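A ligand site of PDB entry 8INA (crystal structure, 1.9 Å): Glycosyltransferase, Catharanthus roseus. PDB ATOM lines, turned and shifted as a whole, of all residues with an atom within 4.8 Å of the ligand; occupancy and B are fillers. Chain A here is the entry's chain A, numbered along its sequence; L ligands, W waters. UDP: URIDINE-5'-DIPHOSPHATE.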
ATOM      1  N   LYS A  23       3.788 -22.793  14.437  1.00  0.00           N
ATOM      2  CA  LYS A  23       4.240 -24.166  14.206  1.00  0.00           C
ATOM      3  C   LYS A  23       3.265 -25.208  14.756  1.00  0.00           C
ATOM      4  O   LYS A  23       3.095 -26.280  14.174  1.00  0.00           O
ATOM      5  CB  LYS A  23       5.648 -24.383  14.795  1.00  0.00           C
ATOM      6  CG  LYS A  23       6.740 -23.639  14.013  1.00  0.00           C
ATOM      7  CD  LYS A  23       8.154 -24.153  14.281  1.00  0.00           C
ATOM      8  CE  LYS A  23       9.189 -23.144  13.775  1.00  0.00           C
ATOM      9  NZ  LYS A  23       8.509 -21.906  13.279  1.00  0.00           N
ATOM     10  N   GLY A  24       2.628 -24.929  15.890  1.00  0.00           N
ATOM     11  CA  GLY A  24       1.640 -25.855  16.425  1.00  0.00           C
ATOM     12  C   GLY A  24       0.358 -25.964  15.585  1.00  0.00           C
ATOM     13  O   GLY A  24      -0.464 -26.845  15.848  1.00  0.00           O
ATOM     14  N   ASN A  27       2.313 -27.739  11.761  1.00  0.00           N
ATOM     15  CA  ASN A  27       2.802 -29.120  11.789  1.00  0.00           C
ATOM     16  C   ASN A  27       1.681 -30.168  11.737  1.00  0.00           C
ATOM     17  O   ASN A  27       1.758 -31.078  10.888  1.00  0.00           O
ATOM     18  CB  ASN A  27       3.725 -29.317  13.008  1.00  0.00           C
ATOM     19  CG  ASN A  27       5.092 -28.616  12.851  1.00  0.00           C
ATOM     20  OD1 ASN A  27       5.413 -28.092  11.787  1.00  0.00           O
ATOM     21  ND2 ASN A  27       5.901 -28.631  13.908  1.00  0.00           N
ATOM     22  N   TYR A 268       9.396 -32.905   8.649  1.00  0.00           N
ATOM     23  CA  TYR A 268       9.696 -31.589   9.200  1.00  0.00           C
ATOM     24  C   TYR A 268       9.918 -30.561   8.098  1.00  0.00           C
ATOM     25  O   TYR A 268      10.559 -30.841   7.085  1.00  0.00           O
ATOM     26  CB  TYR A 268      10.937 -31.651  10.080  1.00  0.00           C
ATOM     27  CG  TYR A 268      10.891 -32.732  11.145  1.00  0.00           C
ATOM     28  CD1 TYR A 268      10.121 -32.571  12.295  1.00  0.00           C
ATOM     29  CD2 TYR A 268      11.627 -33.901  11.010  1.00  0.00           C
ATOM     30  CE1 TYR A 268      10.089 -33.571  13.298  1.00  0.00           C
ATOM     31  CE2 TYR A 268      11.609 -34.895  11.984  1.00  0.00           C
ATOM     32  CZ  TYR A 268      10.840 -34.735  13.133  1.00  0.00           C
ATOM     33  OH  TYR A 268      10.831 -35.727  14.118  1.00  0.00           O
ATOM     34  N   TYR A 291      13.602 -35.239  28.387  1.00  0.00           N
ATOM     35  CA  TYR A 291      13.414 -34.301  27.282  1.00  0.00           C
ATOM     36  C   TYR A 291      12.635 -33.095  27.794  1.00  0.00           C
ATOM     37  O   TYR A 291      11.647 -33.251  28.515  1.00  0.00           O
ATOM     38  CB  TYR A 291      12.680 -34.989  26.128  1.00  0.00           C
ATOM     39  CG  TYR A 291      12.296 -34.086  24.978  1.00  0.00           C
ATOM     40  CD1 TYR A 291      13.227 -33.193  24.439  1.00  0.00           C
ATOM     41  CD2 TYR A 291      11.020 -34.147  24.415  1.00  0.00           C
ATOM     42  CE1 TYR A 291      12.881 -32.361  23.356  1.00  0.00           C
ATOM     43  CE2 TYR A 291      10.662 -33.312  23.350  1.00  0.00           C
ATOM     44  CZ  TYR A 291      11.585 -32.421  22.835  1.00  0.00           C
ATOM     45  OH  TYR A 291      11.200 -31.610  21.776  1.00  0.00           O
ATOM     46  N   SER A 293      11.030 -29.230  26.703  1.00  0.00           N
ATOM     47  CA  SER A 293      10.719 -28.238  25.666  1.00  0.00           C
ATOM     48  C   SER A 293       9.484 -27.434  26.064  1.00  0.00           C
ATOM     49  O   SER A 293       8.507 -27.984  26.561  1.00  0.00           O
ATOM     50  CB  SER A 293      10.460 -28.899  24.306  1.00  0.00           C
ATOM     51  OG  SER A 293      10.010 -27.933  23.366  1.00  0.00           O
ATOM     52  N   GLY A 295       7.984 -25.614  23.616  1.00  0.00           N
ATOM     53  CA  GLY A 295       7.266 -25.400  22.378  1.00  0.00           C
ATOM     54  C   GLY A 295       7.891 -24.319  21.505  1.00  0.00           C
ATOM     55  O   GLY A 295       9.066 -23.970  21.634  1.00  0.00           O
ATOM     56  N   SER A 296       7.070 -23.789  20.591  1.00  0.00           N
ATOM     57  CA  SER A 296       7.530 -22.848  19.567  1.00  0.00           C
ATOM     58  C   SER A 296       7.282 -21.380  19.914  1.00  0.00           C
ATOM     59  O   SER A 296       7.773 -20.517  19.194  1.00  0.00           O
ATOM     60  CB  SER A 296       6.860 -23.152  18.213  1.00  0.00           C
ATOM     61  OG  SER A 296       5.454 -22.866  18.237  1.00  0.00           O
ATOM     62  N   LEU A 297       6.536 -21.091  20.983  1.00  0.00           N
ATOM     63  CA  LEU A 297       6.077 -19.721  21.237  1.00  0.00           C
ATOM     64  C   LEU A 297       6.389 -19.238  22.652  1.00  0.00           C
ATOM     65  O   LEU A 297       6.880 -18.118  22.842  1.00  0.00           O
ATOM     66  CB  LEU A 297       4.576 -19.639  21.019  1.00  0.00           C
ATOM     67  CG  LEU A 297       4.066 -19.681  19.581  1.00  0.00           C
ATOM     68  CD1 LEU A 297       2.534 -19.852  19.564  1.00  0.00           C
ATOM     69  CD2 LEU A 297       4.492 -18.429  18.833  1.00  0.00           C
ATOM     70  N   VAL A 322      15.420 -28.136  24.641  1.00  0.00           N
ATOM     71  CA  VAL A 322      15.233 -27.228  23.506  1.00  0.00           C
ATOM     72  C   VAL A 322      15.098 -25.809  24.056  1.00  0.00           C
ATOM     73  O   VAL A 322      14.133 -25.503  24.775  1.00  0.00           O
ATOM     74  CB  VAL A 322      14.015 -27.620  22.656  1.00  0.00           C
ATOM     75  CG1 VAL A 322      13.777 -26.610  21.536  1.00  0.00           C
ATOM     76  CG2 VAL A 322      14.172 -29.031  22.105  1.00  0.00           C
ATOM     77  N   TRP A 349      16.412 -26.476  18.417  1.00  0.00           N
ATOM     78  CA  TRP A 349      15.225 -27.164  17.892  1.00  0.00           C
ATOM     79  C   TRP A 349      15.632 -28.610  17.638  1.00  0.00           C
ATOM     80  O   TRP A 349      16.788 -28.861  17.283  1.00  0.00           O
ATOM     81  CB  TRP A 349      14.722 -26.527  16.575  1.00  0.00           C
ATOM     82  CG  TRP A 349      13.230 -26.702  16.291  1.00  0.00           C
ATOM     83  CD1 TRP A 349      12.669 -27.334  15.213  1.00  0.00           C
ATOM     84  CD2 TRP A 349      12.142 -26.200  17.073  1.00  0.00           C
ATOM     85  NE1 TRP A 349      11.283 -27.273  15.297  1.00  0.00           N
ATOM     86  CE2 TRP A 349      10.941 -26.584  16.431  1.00  0.00           C
ATOM     87  CE3 TRP A 349      12.061 -25.477  18.268  1.00  0.00           C
ATOM     88  CZ2 TRP A 349       9.677 -26.253  16.935  1.00  0.00           C
ATOM     89  CZ3 TRP A 349      10.808 -25.165  18.777  1.00  0.00           C
ATOM     90  CH2 TRP A 349       9.628 -25.541  18.099  1.00  0.00           C
ATOM     91  N   CYS A 350      14.729 -29.554  17.840  1.00  0.00           N
ATOM     92  CA  CYS A 350      15.053 -30.971  17.694  1.00  0.00           C
ATOM     93  C   CYS A 350      13.991 -31.655  16.847  1.00  0.00           C
ATOM     94  O   CYS A 350      12.962 -31.050  16.519  1.00  0.00           O
ATOM     95  CB  CYS A 350      15.175 -31.646  19.081  1.00  0.00           C
ATOM     96  SG  CYS A 350      13.569 -32.103  19.827  1.00  0.00           S
ATOM     97  N   GLN A 352      11.255 -33.587  17.127  1.00  0.00           N
ATOM     98  CA  GLN A 352      10.533 -33.978  18.345  1.00  0.00           C
ATOM     99  C   GLN A 352       9.888 -35.358  18.199  1.00  0.00           C
ATOM    100  O   GLN A 352       9.817 -36.125  19.170  1.00  0.00           O
ATOM    101  CB  GLN A 352       9.470 -32.930  18.716  1.00  0.00           C
ATOM    102  CG  GLN A 352       8.496 -33.440  19.849  1.00  0.00           C
ATOM    103  CD  GLN A 352       7.816 -32.334  20.658  1.00  0.00           C
ATOM    104  OE1 GLN A 352       6.572 -32.332  20.828  1.00  0.00           O
ATOM    105  NE2 GLN A 352       8.607 -31.390  21.164  1.00  0.00           N
ATOM    106  N   LEU A 353       9.359 -35.680  17.012  1.00  0.00           N
ATOM    107  CA  LEU A 353       8.753 -37.009  16.854  1.00  0.00           C
ATOM    108  C   LEU A 353       9.799 -38.105  17.055  1.00  0.00           C
ATOM    109  O   LEU A 353       9.534 -39.123  17.707  1.00  0.00           O
ATOM    110  CB  LEU A 353       8.102 -37.151  15.477  1.00  0.00           C
ATOM    111  CG  LEU A 353       7.037 -36.117  15.091  1.00  0.00           C
ATOM    112  CD1 LEU A 353       6.483 -36.450  13.704  1.00  0.00           C
ATOM    113  CD2 LEU A 353       5.910 -36.095  16.131  1.00  0.00           C
ATOM    114  N   HIS A 367       5.435 -27.807  28.255  1.00  0.00           N
ATOM    115  CA  HIS A 367       4.446 -26.761  28.484  1.00  0.00           C
ATOM    116  C   HIS A 367       3.027 -27.210  28.189  1.00  0.00           C
ATOM    117  O   HIS A 367       2.092 -26.429  28.420  1.00  0.00           O
ATOM    118  CB  HIS A 367       4.782 -25.507  27.641  1.00  0.00           C
ATOM    119  CG  HIS A 367       4.386 -25.623  26.198  1.00  0.00           C
ATOM    120  ND1 HIS A 367       4.764 -26.695  25.406  1.00  0.00           N
ATOM    121  CD2 HIS A 367       3.698 -24.783  25.386  1.00  0.00           C
ATOM    122  CE1 HIS A 367       4.284 -26.523  24.182  1.00  0.00           C
ATOM    123  NE2 HIS A 367       3.631 -25.375  24.147  1.00  0.00           N
ATOM    124  N   GLY A 369       1.425 -27.873  25.328  1.00  0.00           N
ATOM    125  CA  GLY A 369       0.741 -27.604  24.072  1.00  0.00           C
ATOM    126  C   GLY A 369       0.108 -28.898  23.562  1.00  0.00           C
ATOM    127  O   GLY A 369       0.570 -29.982  23.934  1.00  0.00           O
ATOM    128  N   TRP A 370      -0.953 -28.814  22.751  1.00  0.00           N
ATOM    129  CA  TRP A 370      -1.660 -30.039  22.377  1.00  0.00           C
ATOM    130  C   TRP A 370      -0.803 -30.981  21.529  1.00  0.00           C
ATOM    131  O   TRP A 370      -0.860 -32.204  21.722  1.00  0.00           O
ATOM    132  CB  TRP A 370      -2.970 -29.742  21.646  1.00  0.00           C
ATOM    133  CG  TRP A 370      -3.691 -31.030  21.261  1.00  0.00           C
ATOM    134  CD1 TRP A 370      -4.079 -31.423  20.005  1.00  0.00           C
ATOM    135  CD2 TRP A 370      -4.074 -32.099  22.142  1.00  0.00           C
ATOM    136  NE1 TRP A 370      -4.688 -32.668  20.061  1.00  0.00           N
ATOM    137  CE2 TRP A 370      -4.693 -33.100  21.363  1.00  0.00           C
ATOM    138  CE3 TRP A 370      -3.955 -32.298  23.534  1.00  0.00           C
ATOM    139  CZ2 TRP A 370      -5.197 -34.277  21.913  1.00  0.00           C
ATOM    140  CZ3 TRP A 370      -4.455 -33.488  24.084  1.00  0.00           C
ATOM    141  CH2 TRP A 370      -5.068 -34.456  23.276  1.00  0.00           C
ATOM    142  N   ASN A 371      -0.032 -30.467  20.559  1.00  0.00           N
ATOM    143  CA  ASN A 371       0.775 -31.383  19.759  1.00  0.00           C
ATOM    144  C   ASN A 371       1.770 -32.144  20.624  1.00  0.00           C
ATOM    145  O   ASN A 371       1.947 -33.356  20.468  1.00  0.00           O
ATOM    146  CB  ASN A 371       1.528 -30.618  18.660  1.00  0.00           C
ATOM    147  CG  ASN A 371       0.578 -30.032  17.642  1.00  0.00           C
ATOM    148  OD1 ASN A 371       0.017 -30.744  16.811  1.00  0.00           O
ATOM    149  ND2 ASN A 371       0.351 -28.731  17.726  1.00  0.00           N
ATOM    150  N   SER A 372       2.440 -31.443  21.537  1.00  0.00           N
ATOM    151  CA  SER A 372       3.398 -32.105  22.416  1.00  0.00           C
ATOM    152  C   SER A 372       2.715 -33.125  23.308  1.00  0.00           C
ATOM    153  O   SER A 372       3.232 -34.233  23.540  1.00  0.00           O
ATOM    154  CB  SER A 372       4.152 -31.054  23.237  1.00  0.00           C
ATOM    155  OG  SER A 372       5.093 -30.367  22.390  1.00  0.00           O
ATOM    156  N   GLU A 375       1.621 -36.083  20.997  1.00  0.00           N
ATOM    157  CA  GLU A 375       2.780 -36.822  20.515  1.00  0.00           C
ATOM    158  C   GLU A 375       3.402 -37.653  21.647  1.00  0.00           C
ATOM    159  O   GLU A 375       3.838 -38.793  21.430  1.00  0.00           O
ATOM    160  CB  GLU A 375       3.803 -35.852  19.911  1.00  0.00           C
ATOM    161  CG  GLU A 375       3.289 -35.263  18.559  1.00  0.00           C
ATOM    162  CD  GLU A 375       4.023 -34.005  18.101  1.00  0.00           C
ATOM    163  OE1 GLU A 375       5.030 -33.618  18.733  1.00  0.00           O
ATOM    164  OE2 GLU A 375       3.583 -33.399  17.099  1.00  0.00           O
ATOM    165  N   TRP A 389      -0.029 -20.894  29.056  1.00  0.00           N
ATOM    166  CA  TRP A 389      -1.246 -20.121  28.765  1.00  0.00           C
ATOM    167  C   TRP A 389      -2.134 -20.886  27.784  1.00  0.00           C
ATOM    168  O   TRP A 389      -1.797 -21.963  27.288  1.00  0.00           O
ATOM    169  CB  TRP A 389      -0.903 -18.744  28.200  1.00  0.00           C
ATOM    170  CG  TRP A 389       0.392 -18.702  27.450  1.00  0.00           C
ATOM    171  CD1 TRP A 389       1.605 -18.265  27.914  1.00  0.00           C
ATOM    172  CD2 TRP A 389       0.592 -19.099  26.099  1.00  0.00           C
ATOM    173  NE1 TRP A 389       2.558 -18.368  26.920  1.00  0.00           N
ATOM    174  CE2 TRP A 389       1.962 -18.885  25.798  1.00  0.00           C
ATOM    175  CE3 TRP A 389      -0.240 -19.629  25.106  1.00  0.00           C
ATOM    176  CZ2 TRP A 389       2.513 -19.175  24.551  1.00  0.00           C
ATOM    177  CZ3 TRP A 389       0.311 -19.919  23.859  1.00  0.00           C
ATOM    178  CH2 TRP A 389       1.671 -19.687  23.588  1.00  0.00           C
ATOM    179  N   GLN A 392      -3.057 -24.826  27.369  1.00  0.00           N
ATOM    180  CA  GLN A 392      -2.056 -25.634  28.072  1.00  0.00           C
ATOM    181  C   GLN A 392      -2.492 -25.973  29.488  1.00  0.00           C
ATOM    182  O   GLN A 392      -2.206 -27.058  30.004  1.00  0.00           O
ATOM    183  CB  GLN A 392      -0.719 -24.902  28.089  1.00  0.00           C
ATOM    184  CG  GLN A 392      -0.094 -24.740  26.717  1.00  0.00           C
ATOM    185  CD  GLN A 392       0.761 -23.478  26.594  1.00  0.00           C
ATOM    186  OE1 GLN A 392       1.355 -23.020  27.572  1.00  0.00           O
ATOM    187  NE2 GLN A 392       0.805 -22.909  25.385  1.00  0.00           N
HETATM  188  N1  UDP L   1       8.618 -29.284  17.925  1.00  0.00           N
HETATM  189  C2  UDP L   1       9.679 -29.731  17.266  1.00  0.00           C
HETATM  190  N3  UDP L   1      10.920 -29.605  17.697  1.00  0.00           N
HETATM  191  C4  UDP L   1      11.113 -29.022  18.857  1.00  0.00           C
HETATM  192  C5  UDP L   1      10.045 -28.520  19.616  1.00  0.00           C
HETATM  193  C6  UDP L   1       8.759 -28.674  19.099  1.00  0.00           C
HETATM  194  O2  UDP L   1       9.515 -30.378  16.064  1.00  0.00           O
HETATM  195  O4  UDP L   1      12.398 -28.897  19.309  1.00  0.00           O
HETATM  196  C1' UDP L   1       7.280 -29.394  17.348  1.00  0.00           C
HETATM  197  C2' UDP L   1       6.326 -30.337  18.083  1.00  0.00           C
HETATM  198  O2' UDP L   1       6.481 -31.593  17.580  1.00  0.00           O
HETATM  199  C3' UDP L   1       4.972 -29.689  17.715  1.00  0.00           C
HETATM  200  C4' UDP L   1       5.178 -28.377  17.732  1.00  0.00           C
HETATM  201  O4' UDP L   1       6.747 -28.188  17.488  1.00  0.00           O
HETATM  202  O3' UDP L   1       4.585 -30.086  16.327  1.00  0.00           O
HETATM  203  C5' UDP L   1       4.833 -27.738  19.073  1.00  0.00           C
HETATM  204  O5' UDP L   1       3.443 -27.543  19.095  1.00  0.00           O
HETATM  205  PA  UDP L   1       2.679 -27.521  20.555  1.00  0.00           P
HETATM  206  O1A UDP L   1       1.223 -27.729  20.269  1.00  0.00           O
HETATM  207  O2A UDP L   1       3.241 -28.598  21.455  1.00  0.00           O
HETATM  208  O3A UDP L   1       2.976 -26.113  21.326  1.00  0.00           O
HETATM  209  PB  UDP L   1       3.049 -24.592  20.668  1.00  0.00           P
HETATM  210  O1B UDP L   1       1.906 -24.421  19.676  1.00  0.00           O
HETATM  211  O2B UDP L   1       2.915 -23.709  21.865  1.00  0.00           O
HETATM  212  O3B UDP L   1       4.390 -24.380  19.999  1.00  0.00           O
HETATM  213  O   HOH W   1       4.800 -32.408  14.969  1.00  0.00           O
HETATM  214  O   HOH W   2       5.055 -22.577  22.997  1.00  0.00           O
HETATM  215  O   HOH W   3       7.742 -28.979  22.194  1.00  0.00           O
HETATM  216  O   HOH W   4       1.853 -22.696  17.603  1.00  0.00           O
HETATM  217  O   HOH W   5       7.595 -32.301  14.946  1.00  0.00           O
HETATM  218  O   HOH W   6       8.953 -28.490  13.790  1.00  0.00           O
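The side-chain hydroxyl (OG) of Ser 372 is in hydrogen-bond range of the side-chain amide oxygen (OE1) of Gln 352 (2.9 Å).
OE1 of Gln 352 sits close to OE1 of Glu 375, 2.9 Å away.
The side-chain hydroxyl (OH) of Tyr 291 is in hydrogen-bond range of the side-chain sulfur (SG) of Cys 350, 3.1 Å away.
The side-chain amide nitrogen of Asn 371 sits at hydrogen-bond distance from the backbone carbonyl oxygen of Gly 24, at 2.8 Å.
OH of Tyr 291 is in hydrogen-bond range of NE2 of Gln 352 (2.7 Å).
N of Gly 295 sits at hydrogen-bond distance from OG of Ser 293, 3.1 Å away.
O3B of the ligand sits at hydrogen-bond distance from N of Ser 296 (2.8 Å).
OG of Ser 296 lies within hydrogen-bond range of O3B of the ligand, at 2.6 Å.
An oxygen (O2A) of the ligand sits at hydrogen-bond distance from the backbone NH of Ser 372 (3.0 Å).
O2A of the ligand sits at hydrogen-bond distance from OG of Ser 372 (2.7 Å).
The side-chain carboxylate of Glu 375 is in hydrogen-bond range of an oxygen (O2') of the ligand (2.7 Å).
The backbone NH of Cys 350 lies within hydrogen-bond range of an oxygen (O4) of the ligand, 2.8 Å away.
O of Cys 350 sits at hydrogen-bond distance from N3 of the ligand (2.8 Å).
The side-chain sulfur (SG) of Cys 350 is in hydrogen-bond range of an oxygen (O4) of the ligand, 3.5 Å away.
The backbone NH (N) of Asn 371 is in hydrogen-bond range of an oxygen (O1A) of the ligand, at 3.0 Å.
ND2 of Asn 371 lies within hydrogen-bond range of O1A of the ligand, at 2.9 Å.
NE2 of His 367 lies within hydrogen-bond range of O2B of the ligand (2.9 Å).
O3' of the ligand is in hydrogen-bond range of ND2 of Asn 27, 3.1 Å away.
O2' of the ligand lies within hydrogen-bond range of OE1 of Gln 352 (3.3 Å).
The backbone NH (N) of Trp 370 is in hydrogen-bond range of an oxygen (O1A) of the ligand (3.5 Å).
NE1 of Trp 349 sits close to N3 of the ligand (3.4 Å).
Gly 24 touches the ligand.
OH of Tyr 291 touches O4 of the ligand, at 3.9 Å.
OG of Ser 293 touches C5 of the ligand, at 3.8 Å.
Gly 295 touches the ligand.
CG2 of Val 322 touches O4 of the ligand, 3.3 Å away.
Gly 369 touches the ligand (C to O1A, 3.7 Å).
Hydrophobic or aromatic side chains within 4 Å of the ligand: Val 322, Trp 349 and His 367.
16 residues have an atom within 4 Å of the ligand: Gly 24, Asn 27, Tyr 291, Ser 293, Gly 295, Ser 296, Val 322, Trp 349, Cys 350, Gln 352, His 367, Gly 369, Trp 370, Asn 371, Ser 372 and Glu 375.
The nearest printed residue that does not touch the ligand is Leu 297 (4.05 Å).
Water W2 lies within hydrogen-bond range of an oxygen (O2B) of the ligand, the backbone NH (N) of Leu 297, a ring nitrogen (NE2) of His 367 and the backbone NH (N) of Ser 296.
Water W4 lies within hydrogen-bond range of an oxygen (O1B) of the ligand (2.7 Å) and the backbone NH (N) of Gly 24 (2.9 Å).
Water W1 bridges the side-chain carboxylate of Glu 375 and an oxygen (O3') of the ligand.
Water W6 lies within hydrogen-bond range of an oxygen (O2) of the ligand (3.0 Å), the indole nitrogen (NE1) of Trp 349 (3.0 Å) and the side-chain amide nitrogen (ND2) of Asn 27 (3.1 Å).
Water W3 lies within hydrogen-bond range of the side-chain hydroxyl of Ser 293, the side-chain amide nitrogen of Gln 352 and the side-chain hydroxyl of Ser 372.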
